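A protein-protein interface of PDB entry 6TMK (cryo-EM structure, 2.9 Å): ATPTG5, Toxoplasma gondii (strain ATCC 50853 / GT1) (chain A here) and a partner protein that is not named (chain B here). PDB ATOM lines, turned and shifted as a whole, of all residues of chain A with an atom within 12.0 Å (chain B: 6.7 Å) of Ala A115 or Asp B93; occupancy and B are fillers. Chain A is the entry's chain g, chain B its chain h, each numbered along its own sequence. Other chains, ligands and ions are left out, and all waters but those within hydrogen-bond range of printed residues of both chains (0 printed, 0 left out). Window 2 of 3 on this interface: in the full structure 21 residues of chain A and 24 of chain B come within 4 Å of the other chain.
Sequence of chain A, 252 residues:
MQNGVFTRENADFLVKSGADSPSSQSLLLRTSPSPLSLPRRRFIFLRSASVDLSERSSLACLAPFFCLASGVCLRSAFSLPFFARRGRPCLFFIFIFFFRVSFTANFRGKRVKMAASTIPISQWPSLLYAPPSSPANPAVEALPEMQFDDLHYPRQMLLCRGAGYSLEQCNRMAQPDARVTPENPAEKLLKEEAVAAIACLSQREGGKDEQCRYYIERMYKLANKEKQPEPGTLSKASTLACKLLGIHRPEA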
ATOM      1  N   ALA A 115      25.653 -30.416 -21.415  1.00  0.00           N
ATOM      2  CA  ALA A 115      24.896 -31.612 -21.758  1.00  0.00           C
ATOM      3  C   ALA A 115      23.564 -31.628 -21.022  1.00  0.00           C
ATOM      4  O   ALA A 115      22.508 -31.777 -21.635  1.00  0.00           O
ATOM      5  CB  ALA A 115      25.696 -32.861 -21.433  1.00  0.00           C
ATOM      6  N   ALA A 116      23.620 -31.478 -19.701  1.00  0.00           N
ATOM      7  CA  ALA A 116      22.415 -31.363 -18.886  1.00  0.00           C
ATOM      8  C   ALA A 116      21.860 -29.959 -19.051  1.00  0.00           C
ATOM      9  O   ALA A 116      22.328 -29.010 -18.420  1.00  0.00           O
ATOM     10  CB  ALA A 116      22.722 -31.667 -17.427  1.00  0.00           C
ATOM     11  N   SER A 117      20.856 -29.825 -19.904  1.00  0.00           N
ATOM     12  CA  SER A 117      20.290 -28.529 -20.229  1.00  0.00           C
ATOM     13  C   SER A 117      19.159 -28.183 -19.270  1.00  0.00           C
ATOM     14  O   SER A 117      18.580 -29.046 -18.608  1.00  0.00           O
ATOM     15  CB  SER A 117      19.790 -28.508 -21.671  1.00  0.00           C
ATOM     16  OG  SER A 117      19.079 -29.690 -21.980  1.00  0.00           O
ATOM     17  N   THR A 118      18.845 -26.896 -19.213  1.00  0.00           N
ATOM     18  CA  THR A 118      17.831 -26.408 -18.293  1.00  0.00           C
ATOM     19  C   THR A 118      16.451 -26.938 -18.660  1.00  0.00           C
ATOM     20  O   THR A 118      16.089 -27.027 -19.835  1.00  0.00           O
ATOM     21  CB  THR A 118      17.817 -24.884 -18.295  1.00  0.00           C
ATOM     22  OG1 THR A 118      19.161 -24.394 -18.308  1.00  0.00           O
ATOM     23  CG2 THR A 118      17.111 -24.356 -17.087  1.00  0.00           C
ATOM     24  N   ILE A 119      15.679 -27.279 -17.633  1.00  0.00           N
ATOM     25  CA  ILE A 119      14.303 -27.738 -17.785  1.00  0.00           C
ATOM     26  C   ILE A 119      13.395 -26.543 -17.508  1.00  0.00           C
ATOM     27  O   ILE A 119      13.368 -26.057 -16.366  1.00  0.00           O
ATOM     28  CB  ILE A 119      13.981 -28.900 -16.837  1.00  0.00           C
ATOM     29  CG1 ILE A 119      15.098 -29.939 -16.841  1.00  0.00           C
ATOM     30  CG2 ILE A 119      12.667 -29.544 -17.221  1.00  0.00           C
ATOM     31  CD1 ILE A 119      15.459 -30.443 -18.184  1.00  0.00           C
ATOM     32  N   PRO A 120      12.660 -26.037 -18.491  1.00  0.00           N
ATOM     33  CA  PRO A 120      11.771 -24.907 -18.220  1.00  0.00           C
ATOM     34  C   PRO A 120      10.645 -25.304 -17.280  1.00  0.00           C
ATOM     35  O   PRO A 120      10.431 -26.474 -16.962  1.00  0.00           O
ATOM     36  CB  PRO A 120      11.240 -24.529 -19.605  1.00  0.00           C
ATOM     37  CG  PRO A 120      12.200 -25.119 -20.551  1.00  0.00           C
ATOM     38  CD  PRO A 120      12.672 -26.372 -19.920  1.00  0.00           C
ATOM     39  N   GLN A 123       7.879 -27.935 -18.164  1.00  0.00           N
ATOM     40  CA  GLN A 123       8.254 -29.334 -18.256  1.00  0.00           C
ATOM     41  C   GLN A 123       8.427 -29.991 -16.897  1.00  0.00           C
ATOM     42  O   GLN A 123       8.827 -31.155 -16.833  1.00  0.00           O
ATOM     43  CB  GLN A 123       9.543 -29.468 -19.063  1.00  0.00           C
ATOM     44  CG  GLN A 123       9.340 -29.492 -20.554  1.00  0.00           C
ATOM     45  CD  GLN A 123      10.622 -29.755 -21.314  1.00  0.00           C
ATOM     46  OE1 GLN A 123      11.716 -29.675 -20.755  1.00  0.00           O
ATOM     47  NE2 GLN A 123      10.496 -30.081 -22.593  1.00  0.00           N
ATOM     48  N   PRO A 132      15.425 -37.270 -14.379  1.00  0.00           N
ATOM     49  CA  PRO A 132      16.620 -37.714 -15.096  1.00  0.00           C
ATOM     50  C   PRO A 132      17.370 -38.783 -14.320  1.00  0.00           C
ATOM     51  O   PRO A 132      17.086 -39.075 -13.158  1.00  0.00           O
ATOM     52  CB  PRO A 132      17.443 -36.433 -15.225  1.00  0.00           C
ATOM     53  CG  PRO A 132      17.000 -35.607 -14.087  1.00  0.00           C
ATOM     54  CD  PRO A 132      15.548 -35.871 -13.949  1.00  0.00           C
ATOM     55  N   SER A 133      18.354 -39.369 -14.994  1.00  0.00           N
ATOM     56  CA  SER A 133      19.119 -40.459 -14.414  1.00  0.00           C
ATOM     57  C   SER A 133      20.130 -39.938 -13.406  1.00  0.00           C
ATOM     58  O   SER A 133      20.727 -38.874 -13.587  1.00  0.00           O
ATOM     59  CB  SER A 133      19.827 -41.250 -15.510  1.00  0.00           C
ATOM     60  OG  SER A 133      18.888 -41.823 -16.400  1.00  0.00           O
ATOM     61  N   GLU B  48      28.971 -23.386  -8.263  1.00  0.00           N
ATOM     62  CA  GLU B  48      28.543 -22.084  -8.747  1.00  0.00           C
ATOM     63  C   GLU B  48      27.537 -21.524  -7.756  1.00  0.00           C
ATOM     64  O   GLU B  48      26.417 -22.049  -7.670  1.00  0.00           O
ATOM     65  CB  GLU B  48      27.925 -22.196 -10.135  1.00  0.00           C
ATOM     66  CG  GLU B  48      28.128 -20.967 -10.992  1.00  0.00           C
ATOM     67  CD  GLU B  48      27.166 -20.903 -12.159  1.00  0.00           C
ATOM     68  OE1 GLU B  48      26.456 -21.900 -12.401  1.00  0.00           O
ATOM     69  OE2 GLU B  48      27.115 -19.852 -12.831  1.00  0.00           O
ATOM     70  N   PRO B  90      20.955 -18.755 -18.109  1.00  0.00           N
ATOM     71  CA  PRO B  90      21.583 -19.870 -17.402  1.00  0.00           C
ATOM     72  C   PRO B  90      22.731 -20.476 -18.193  1.00  0.00           C
ATOM     73  O   PRO B  90      22.803 -20.391 -19.420  1.00  0.00           O
ATOM     74  CB  PRO B  90      20.440 -20.876 -17.245  1.00  0.00           C
ATOM     75  CG  PRO B  90      19.519 -20.565 -18.353  1.00  0.00           C
ATOM     76  CD  PRO B  90      19.610 -19.098 -18.594  1.00  0.00           C
ATOM     77  N   GLU B  91      23.641 -21.101 -17.453  1.00  0.00           N
ATOM     78  CA  GLU B  91      24.755 -21.791 -18.074  1.00  0.00           C
ATOM     79  C   GLU B  91      24.273 -23.023 -18.835  1.00  0.00           C
ATOM     80  O   GLU B  91      23.188 -23.556 -18.595  1.00  0.00           O
ATOM     81  CB  GLU B  91      25.791 -22.182 -17.023  1.00  0.00           C
ATOM     82  CG  GLU B  91      25.252 -23.026 -15.888  1.00  0.00           C
ATOM     83  CD  GLU B  91      26.336 -23.470 -14.927  1.00  0.00           C
ATOM     84  OE1 GLU B  91      27.510 -23.108 -15.145  1.00  0.00           O
ATOM     85  OE2 GLU B  91      26.013 -24.179 -13.951  1.00  0.00           O
ATOM     86  N   ALA B  92      25.106 -23.468 -19.773  1.00  0.00           N
ATOM     87  CA  ALA B  92      24.739 -24.595 -20.620  1.00  0.00           C
ATOM     88  C   ALA B  92      24.633 -25.877 -19.808  1.00  0.00           C
ATOM     89  O   ALA B  92      23.650 -26.617 -19.920  1.00  0.00           O
ATOM     90  CB  ALA B  92      25.758 -24.756 -21.742  1.00  0.00           C
ATOM     91  N   ASP B  93      25.642 -26.158 -18.991  1.00  0.00           N
ATOM     92  CA  ASP B  93      25.674 -27.359 -18.172  1.00  0.00           C
ATOM     93  C   ASP B  93      25.114 -27.030 -16.795  1.00  0.00           C
ATOM     94  O   ASP B  93      25.659 -26.186 -16.075  1.00  0.00           O
ATOM     95  CB  ASP B  93      27.095 -27.910 -18.084  1.00  0.00           C
ATOM     96  CG  ASP B  93      27.134 -29.366 -17.666  1.00  0.00           C
ATOM     97  OD1 ASP B  93      26.076 -30.029 -17.700  1.00  0.00           O
ATOM     98  OD2 ASP B  93      28.226 -29.856 -17.315  1.00  0.00           O
ATOM     99  N   ARG B  94      24.026 -27.706 -16.438  1.00  0.00           N
ATOM    100  CA  ARG B  94      23.235 -27.449 -15.238  1.00  0.00           C
ATOM    101  C   ARG B  94      23.139 -28.753 -14.455  1.00  0.00           C
ATOM    102  O   ARG B  94      22.065 -29.269 -14.150  1.00  0.00           O
ATOM    103  CB  ARG B  94      21.863 -26.871 -15.585  1.00  0.00           C
ATOM    104  CG  ARG B  94      21.864 -25.358 -15.717  1.00  0.00           C
ATOM    105  CD  ARG B  94      20.493 -24.735 -15.497  1.00  0.00           C
ATOM    106  NE  ARG B  94      20.090 -24.672 -14.098  1.00  0.00           N
ATOM    107  CZ  ARG B  94      20.652 -23.876 -13.201  1.00  0.00           C
ATOM    108  NH1 ARG B  94      21.640 -23.073 -13.551  1.00  0.00           N
ATOM    109  NH2 ARG B  94      20.220 -23.879 -11.953  1.00  0.00           N
ATOM    110  N   ILE B  95      24.317 -29.275 -14.128  1.00  0.00           N
ATOM    111  CA  ILE B  95      24.583 -30.678 -13.843  1.00  0.00           C
ATOM    112  C   ILE B  95      23.436 -31.330 -13.091  1.00  0.00           C
ATOM    113  O   ILE B  95      23.029 -32.450 -13.416  1.00  0.00           O
ATOM    114  CB  ILE B  95      25.890 -30.791 -13.038  1.00  0.00           C
ATOM    115  CG1 ILE B  95      27.072 -30.361 -13.891  1.00  0.00           C
ATOM    116  CG2 ILE B  95      26.101 -32.196 -12.550  1.00  0.00           C
ATOM    117  CD1 ILE B  95      28.068 -29.554 -13.148  1.00  0.00           C
ATOM    118  N   ASN B  96      22.906 -30.644 -12.088  1.00  0.00           N
ATOM    119  CA  ASN B  96      21.721 -31.103 -11.379  1.00  0.00           C
ATOM    120  C   ASN B  96      20.486 -30.567 -12.087  1.00  0.00           C
ATOM    121  O   ASN B  96      20.184 -29.373 -12.008  1.00  0.00           O
ATOM    122  CB  ASN B  96      21.750 -30.649  -9.927  1.00  0.00           C
ATOM    123  CG  ASN B  96      20.740 -31.364  -9.077  1.00  0.00           C
ATOM    124  OD1 ASN B  96      19.836 -32.018  -9.586  1.00  0.00           O
ATOM    125  ND2 ASN B  96      20.884 -31.241  -7.771  1.00  0.00           N
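The side-chain carboxylate of Asp B93 sits at hydrogen-bond distance from the backbone NH of Ala A116. The backbone NH of Arg B94 lies within hydrogen-bond range of the backbone carbonyl oxygen of Ala A116 (2.9 Å). O of Ala A116 lies close to O of Ala B92 (3.1 Å).
Ala A115 touches Asp B93 (N to OD1, 3.8 Å). Ser A117 touches Ala B92 (CA to O, 3.9 Å). Thr A118 touches Pro B90. OG1 of Thr A118 touches CD of Arg B94 (3.1 Å).
Of chain B, only Asp B93 (3.8 Å) comes within 4 Å of Ala A115. Printed residues of chain B within 4 Å of Ala A116: Ala B92, Asp B93 and Arg B94. Of the printed residues of chain B, Ser A117 touches Ala B92. Of the printed residues of chain B, Thr A118 touches Pro B90 (3.8 Å) and Arg B94 (3.1 Å). Of the printed residues of chain A, Pro B90 touches Thr A118. No residue of chain A comes within 4 Å of Glu B91. Ala B92 touches two residues of chain A. Asp B93 touches just these residues of chain A: Ala A115 (3.8 Å) and Ala A116 (3.5 Å). Of chain A, only Ala A116 (2.9 Å) and Thr A118 (3.1 Å) come within 4 Å of Arg B94. No residue of chain A comes within 4 Å of Ile B95. The nearest residue of chain B that does not touch Ala A115 is Ala B92 (4.5 Å). The nearest residue of chain A that does not touch Asp B93 is Ser A117 (5.7 Å).
Hydrophobic or aromatic side chains of chain A that line the printed part of chain B: Ala A116. Printed residues of chain B that touch a printed residue of chain A: Pro B90, Ala B92, Asp B93 and Arg B94. Hydrophobic or aromatic side chains of chain B that line the printed part of chain A: Pro B90. Among the printed residues, no Asp or Glu carboxylate lies within 4 Å of a Lys or Arg side-chain nitrogen of the other chain.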
